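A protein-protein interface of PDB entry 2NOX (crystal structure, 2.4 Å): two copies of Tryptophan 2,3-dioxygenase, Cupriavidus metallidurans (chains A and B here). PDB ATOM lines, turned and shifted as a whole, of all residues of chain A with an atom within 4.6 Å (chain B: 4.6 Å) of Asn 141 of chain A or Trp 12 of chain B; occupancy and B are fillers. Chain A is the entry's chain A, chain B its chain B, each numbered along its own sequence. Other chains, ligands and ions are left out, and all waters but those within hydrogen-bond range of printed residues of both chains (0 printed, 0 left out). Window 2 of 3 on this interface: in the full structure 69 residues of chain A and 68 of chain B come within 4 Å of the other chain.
No position is printed for both chains.
Of the 10 pairs that touch across the chains among the printed residues, none has its exchanged pair printed and touching as well.
The backbone carbonyl oxygen (O) of Arg 146 of chain A sits close to the backbone carbonyl oxygen (O) of Met 17 of chain B, 3.3 Å away.
The indole nitrogen of Trp 12 of chain B sits at hydrogen-bond distance from the side-chain hydroxyl of Tyr 261 of chain A.
Asn 141 of chain A touches one residue of chain B.
Printed residues of chain A within 4 Å of Trp 12 of chain B: Phe 125, Asn 141, Met 144, Arg 146, Tyr 261 and Met 265.
Of the printed residues of chain A, Met 17 of chain B touches Ala 143 (3.8 Å) and Arg 146 (3.3 Å).
Printed residues of chain B within 4 Å of Phe 125 of chain A: Trp 12 (3.6 Å) and Ala 15 (3.4 Å).
Of the printed residues of chain B, Met 144 of chain A touches Trp 12 (3.9 Å).
Gly 14 of chain B touches none of the printed residues of chain A.
Lys 140 of chain A touches none of the printed residues of chain B.
The nearest printed residue of chain B that does not touch Asn 141 of chain A is His 13 of chain B (6.9 Å).
Among the printed residues, pairs that only touch across the chains: Phe 125 of chain A with Trp 12 of chain B (3.6 Å), Phe 125 of chain A with Ala 15 of chain B (3.4 Å), Asn 141 of chain A with Trp 12 of chain B (3.1 Å), Ala 143 of chain A with Met 17 of chain B (3.8 Å), Met 144 of chain A with Trp 12 of chain B (3.9 Å), Arg 146 of chain A with Trp 12 of chain B (3.9 Å), Tyr 261 of chain A with His 13 of chain B (3.7 Å) and Met 265 of chain A with Trp 12 of chain B (3.96 Å).
Hydrophobic or aromatic side chains of chain B within 4 Å of the printed part of chain A: Trp 12, His 13, Ala 15 and Met 17.
Among the printed residues, 10 pairs touch across the chains.
Among the printed residues, no Asp or Glu carboxylate lies within 4 Å of a Lys or Arg side-chain nitrogen of the other chain.
The backbone NH (N) of Ala 143 of chain A sits at hydrogen-bond distance from the side-chain amide oxygen (OD1) of Asn 141 of chain A, at 2.9 Å.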
ATOM      1  N   PHE A 125     -14.725  11.579 -19.891  1.00  0.00           N
ATOM      2  CA  PHE A 125     -13.767  10.719 -20.572  1.00  0.00           C
ATOM      3  C   PHE A 125     -12.654  10.296 -19.609  1.00  0.00           C
ATOM      4  O   PHE A 125     -12.099   9.207 -19.725  1.00  0.00           O
ATOM      5  CB  PHE A 125     -13.191  11.437 -21.784  1.00  0.00           C
ATOM      6  CG  PHE A 125     -12.534  10.527 -22.775  1.00  0.00           C
ATOM      7  CD1 PHE A 125     -11.154  10.341 -22.765  1.00  0.00           C
ATOM      8  CD2 PHE A 125     -13.284   9.873 -23.720  1.00  0.00           C
ATOM      9  CE1 PHE A 125     -10.544   9.525 -23.679  1.00  0.00           C
ATOM     10  CE2 PHE A 125     -12.678   9.053 -24.657  1.00  0.00           C
ATOM     11  CZ  PHE A 125     -11.303   8.874 -24.633  1.00  0.00           C
ATOM     12  N   PHE A 135     -13.900  -2.315 -17.798  1.00  0.00           N
ATOM     13  CA  PHE A 135     -12.906  -3.395 -17.795  1.00  0.00           C
ATOM     14  C   PHE A 135     -13.435  -4.647 -17.119  1.00  0.00           C
ATOM     15  O   PHE A 135     -13.384  -5.728 -17.684  1.00  0.00           O
ATOM     16  CB  PHE A 135     -11.639  -2.932 -17.088  1.00  0.00           C
ATOM     17  CG  PHE A 135     -10.815  -1.992 -17.911  1.00  0.00           C
ATOM     18  CD1 PHE A 135     -11.252  -1.588 -19.152  1.00  0.00           C
ATOM     19  CD2 PHE A 135      -9.602  -1.501 -17.444  1.00  0.00           C
ATOM     20  CE1 PHE A 135     -10.514  -0.694 -19.914  1.00  0.00           C
ATOM     21  CE2 PHE A 135      -8.866  -0.627 -18.220  1.00  0.00           C
ATOM     22  CZ  PHE A 135      -9.339  -0.234 -19.464  1.00  0.00           C
ATOM     23  N   ASN A 139     -15.006  -4.957 -21.464  1.00  0.00           N
ATOM     24  CA  ASN A 139     -14.794  -3.946 -22.491  1.00  0.00           C
ATOM     25  C   ASN A 139     -13.417  -3.366 -22.301  1.00  0.00           C
ATOM     26  O   ASN A 139     -13.267  -2.209 -21.928  1.00  0.00           O
ATOM     27  CB  ASN A 139     -15.821  -2.819 -22.370  1.00  0.00           C
ATOM     28  CG  ASN A 139     -15.777  -1.859 -23.562  1.00  0.00           C
ATOM     29  OD1 ASN A 139     -15.239  -2.174 -24.619  1.00  0.00           O
ATOM     30  ND2 ASN A 139     -16.344  -0.702 -23.388  1.00  0.00           N
ATOM     31  N   LYS A 140     -12.408  -4.201 -22.533  1.00  0.00           N
ATOM     32  CA  LYS A 140     -11.014  -3.821 -22.341  1.00  0.00           C
ATOM     33  C   LYS A 140     -10.492  -3.003 -23.533  1.00  0.00           C
ATOM     34  O   LYS A 140     -10.812  -3.258 -24.708  1.00  0.00           O
ATOM     35  CB  LYS A 140     -10.128  -5.067 -22.110  1.00  0.00           C
ATOM     36  CG  LYS A 140     -10.543  -5.956 -20.958  1.00  0.00           C
ATOM     37  CD  LYS A 140     -10.055  -5.395 -19.614  1.00  0.00           C
ATOM     38  CE  LYS A 140     -10.236  -6.431 -18.473  1.00  0.00           C
ATOM     39  NZ  LYS A 140      -9.672  -7.785 -18.861  1.00  0.00           N
ATOM     40  N   ASN A 141      -9.677  -2.012 -23.205  1.00  0.00           N
ATOM     41  CA  ASN A 141      -9.163  -1.078 -24.174  1.00  0.00           C
ATOM     42  C   ASN A 141      -7.908  -0.398 -23.623  1.00  0.00           C
ATOM     43  O   ASN A 141      -7.994   0.452 -22.729  1.00  0.00           O
ATOM     44  CB  ASN A 141     -10.235  -0.023 -24.493  1.00  0.00           C
ATOM     45  CG  ASN A 141      -9.793   0.943 -25.582  1.00  0.00           C
ATOM     46  OD1 ASN A 141      -8.599   1.078 -25.853  1.00  0.00           O
ATOM     47  ND2 ASN A 141     -10.751   1.619 -26.204  1.00  0.00           N
ATOM     48  N   ALA A 142      -6.741  -0.780 -24.140  1.00  0.00           N
ATOM     49  CA  ALA A 142      -5.481  -0.225 -23.615  1.00  0.00           C
ATOM     50  C   ALA A 142      -5.371   1.310 -23.818  1.00  0.00           C
ATOM     51  O   ALA A 142      -4.825   2.026 -22.966  1.00  0.00           O
ATOM     52  CB  ALA A 142      -4.270  -0.940 -24.207  1.00  0.00           C
ATOM     53  N   ALA A 143      -5.903   1.810 -24.938  1.00  0.00           N
ATOM     54  CA  ALA A 143      -5.898   3.257 -25.181  1.00  0.00           C
ATOM     55  C   ALA A 143      -6.498   4.012 -24.020  1.00  0.00           C
ATOM     56  O   ALA A 143      -6.196   5.174 -23.812  1.00  0.00           O
ATOM     57  CB  ALA A 143      -6.624   3.617 -26.437  1.00  0.00           C
ATOM     58  N   MET A 144      -7.356   3.367 -23.252  1.00  0.00           N
ATOM     59  CA  MET A 144      -8.043   4.066 -22.185  1.00  0.00           C
ATOM     60  C   MET A 144      -7.223   4.244 -20.927  1.00  0.00           C
ATOM     61  O   MET A 144      -7.730   4.726 -19.920  1.00  0.00           O
ATOM     62  CB  MET A 144      -9.390   3.427 -21.849  1.00  0.00           C
ATOM     63  CG  MET A 144     -10.417   3.529 -22.981  1.00  0.00           C
ATOM     64  SD  MET A 144     -10.756   5.233 -23.517  1.00  0.00           S
ATOM     65  CE  MET A 144     -10.619   6.033 -21.946  1.00  0.00           C
ATOM     66  N   LEU A 145      -5.949   3.872 -20.968  1.00  0.00           N
ATOM     67  CA  LEU A 145      -5.091   4.164 -19.814  1.00  0.00           C
ATOM     68  C   LEU A 145      -4.449   5.563 -19.894  1.00  0.00           C
ATOM     69  O   LEU A 145      -4.174   6.182 -18.856  1.00  0.00           O
ATOM     70  CB  LEU A 145      -3.976   3.135 -19.604  1.00  0.00           C
ATOM     71  CG  LEU A 145      -4.147   1.624 -19.756  1.00  0.00           C
ATOM     72  CD1 LEU A 145      -2.968   0.971 -19.068  1.00  0.00           C
ATOM     73  CD2 LEU A 145      -5.463   1.082 -19.198  1.00  0.00           C
ATOM     74  N   ARG A 146      -4.161   6.044 -21.102  1.00  0.00           N
ATOM     75  CA  ARG A 146      -3.516   7.348 -21.220  1.00  0.00           C
ATOM     76  C   ARG A 146      -4.185   8.552 -20.488  1.00  0.00           C
ATOM     77  O   ARG A 146      -3.473   9.339 -19.857  1.00  0.00           O
ATOM     78  CB  ARG A 146      -3.110   7.680 -22.663  1.00  0.00           C
ATOM     79  CG  ARG A 146      -3.525   6.671 -23.748  1.00  0.00           C
ATOM     80  CD  ARG A 146      -2.711   6.943 -25.040  1.00  0.00           C
ATOM     81  NE  ARG A 146      -3.485   7.010 -26.293  1.00  0.00           N
ATOM     82  CZ  ARG A 146      -3.633   6.009 -27.171  1.00  0.00           C
ATOM     83  NH1 ARG A 146      -3.089   4.812 -26.943  1.00  0.00           N
ATOM     84  NH2 ARG A 146      -4.345   6.203 -28.283  1.00  0.00           N
ATOM     85  N   LEU A 162      -7.112  -3.687 -16.441  1.00  0.00           N
ATOM     86  CA  LEU A 162      -6.937  -4.149 -17.842  1.00  0.00           C
ATOM     87  C   LEU A 162      -6.404  -5.571 -17.867  1.00  0.00           C
ATOM     88  O   LEU A 162      -6.804  -6.387 -18.695  1.00  0.00           O
ATOM     89  CB  LEU A 162      -5.958  -3.240 -18.611  1.00  0.00           C
ATOM     90  CG  LEU A 162      -5.764  -3.472 -20.124  1.00  0.00           C
ATOM     91  CD1 LEU A 162      -6.976  -2.968 -20.987  1.00  0.00           C
ATOM     92  CD2 LEU A 162      -4.464  -2.853 -20.644  1.00  0.00           C
ATOM     93  N   THR A 192      -6.140  -8.200 -21.801  1.00  0.00           N
ATOM     94  CA  THR A 192      -6.173  -6.776 -22.153  1.00  0.00           C
ATOM     95  C   THR A 192      -6.904  -6.545 -23.482  1.00  0.00           C
ATOM     96  O   THR A 192      -7.094  -5.410 -23.905  1.00  0.00           O
ATOM     97  CB  THR A 192      -4.755  -6.207 -22.351  1.00  0.00           C
ATOM     98  OG1 THR A 192      -4.177  -6.772 -23.538  1.00  0.00           O
ATOM     99  CG2 THR A 192      -3.847  -6.481 -21.144  1.00  0.00           C
ATOM    100  N   TYR A 261     -19.494  10.255 -30.768  1.00  0.00           N
ATOM    101  CA  TYR A 261     -18.640   9.322 -30.062  1.00  0.00           C
ATOM    102  C   TYR A 261     -19.460   8.464 -29.106  1.00  0.00           C
ATOM    103  O   TYR A 261     -19.384   7.257 -29.131  1.00  0.00           O
ATOM    104  CB  TYR A 261     -17.568  10.102 -29.318  1.00  0.00           C
ATOM    105  CG  TYR A 261     -16.825   9.283 -28.318  1.00  0.00           C
ATOM    106  CD1 TYR A 261     -15.956   8.254 -28.721  1.00  0.00           C
ATOM    107  CD2 TYR A 261     -16.994   9.519 -26.960  1.00  0.00           C
ATOM    108  CE1 TYR A 261     -15.276   7.481 -27.768  1.00  0.00           C
ATOM    109  CE2 TYR A 261     -16.320   8.763 -26.004  1.00  0.00           C
ATOM    110  CZ  TYR A 261     -15.473   7.750 -26.410  1.00  0.00           C
ATOM    111  OH  TYR A 261     -14.819   7.054 -25.435  1.00  0.00           O
ATOM    112  N   MET A 265     -20.225   4.248 -28.815  1.00  0.00           N
ATOM    113  CA  MET A 265     -20.073   3.347 -27.696  1.00  0.00           C
ATOM    114  C   MET A 265     -21.374   2.664 -27.266  1.00  0.00           C
ATOM    115  O   MET A 265     -21.315   1.625 -26.622  1.00  0.00           O
ATOM    116  CB  MET A 265     -19.345   4.028 -26.532  1.00  0.00           C
ATOM    117  CG  MET A 265     -18.164   4.907 -26.918  1.00  0.00           C
ATOM    118  SD  MET A 265     -16.555   4.114 -27.238  1.00  0.00           S
ATOM    119  CE  MET A 265     -16.543   3.887 -29.019  1.00  0.00           C
ATOM    120  N   TRP B  12      -7.512   8.275 -29.053  1.00  0.00           N
ATOM    121  CA  TRP B  12      -8.765   7.475 -29.238  1.00  0.00           C
ATOM    122  C   TRP B  12      -9.971   8.417 -29.420  1.00  0.00           C
ATOM    123  O   TRP B  12     -10.623   8.818 -28.451  1.00  0.00           O
ATOM    124  CB  TRP B  12      -8.922   6.479 -28.075  1.00  0.00           C
ATOM    125  CG  TRP B  12     -10.270   5.833 -27.890  1.00  0.00           C
ATOM    126  CD1 TRP B  12     -11.344   6.351 -27.216  1.00  0.00           C
ATOM    127  CD2 TRP B  12     -10.671   4.524 -28.334  1.00  0.00           C
ATOM    128  NE1 TRP B  12     -12.401   5.458 -27.235  1.00  0.00           N
ATOM    129  CE2 TRP B  12     -12.018   4.334 -27.919  1.00  0.00           C
ATOM    130  CE3 TRP B  12     -10.034   3.507 -29.062  1.00  0.00           C
ATOM    131  CZ2 TRP B  12     -12.735   3.166 -28.206  1.00  0.00           C
ATOM    132  CZ3 TRP B  12     -10.747   2.353 -29.356  1.00  0.00           C
ATOM    133  CH2 TRP B  12     -12.087   2.189 -28.923  1.00  0.00           C
ATOM    134  N   HIS B  13     -10.211   8.790 -30.684  1.00  0.00           N
ATOM    135  CA  HIS B  13     -11.344   9.642 -31.148  1.00  0.00           C
ATOM    136  C   HIS B  13     -11.197  11.146 -30.946  1.00  0.00           C
ATOM    137  O   HIS B  13     -12.198  11.845 -30.769  1.00  0.00           O
ATOM    138  CB  HIS B  13     -12.695   9.172 -30.591  1.00  0.00           C
ATOM    139  CG  HIS B  13     -13.131   7.838 -31.110  1.00  0.00           C
ATOM    140  ND1 HIS B  13     -12.687   6.648 -30.571  1.00  0.00           N
ATOM    141  CD2 HIS B  13     -13.967   7.503 -32.121  1.00  0.00           C
ATOM    142  CE1 HIS B  13     -13.234   5.636 -31.224  1.00  0.00           C
ATOM    143  NE2 HIS B  13     -14.020   6.127 -32.166  1.00  0.00           N
ATOM    144  N   GLY B  14      -9.963  11.646 -30.993  1.00  0.00           N
ATOM    145  CA  GLY B  14      -9.705  13.083 -30.846  1.00  0.00           C
ATOM    146  C   GLY B  14      -9.781  13.544 -29.400  1.00  0.00           C
ATOM    147  O   GLY B  14      -9.677  14.747 -29.096  1.00  0.00           O
ATOM    148  N   ALA B  15      -9.964  12.587 -28.494  1.00  0.00           N
ATOM    149  CA  ALA B  15     -10.015  12.915 -27.076  1.00  0.00           C
ATOM    150  C   ALA B  15      -8.635  13.341 -26.550  1.00  0.00           C
ATOM    151  O   ALA B  15      -7.614  12.761 -26.914  1.00  0.00           O
ATOM    152  CB  ALA B  15     -10.546  11.748 -26.299  1.00  0.00           C
ATOM    153  N   MET B  17      -5.756  13.207 -24.195  1.00  0.00           N
ATOM    154  CA  MET B  17      -5.211  12.154 -23.348  1.00  0.00           C
ATOM    155  C   MET B  17      -4.391  12.745 -22.198  1.00  0.00           C
ATOM    156  O   MET B  17      -4.402  12.209 -21.089  1.00  0.00           O
ATOM    157  CB  MET B  17      -4.354  11.183 -24.167  1.00  0.00           C
ATOM    158  CG  MET B  17      -5.105  10.315 -25.183  1.00  0.00           C
ATOM    159  SD  MET B  17      -6.588   9.586 -24.481  1.00  0.00           S
ATOM    160  CE  MET B  17      -7.031   8.347 -25.664  1.00  0.00           C
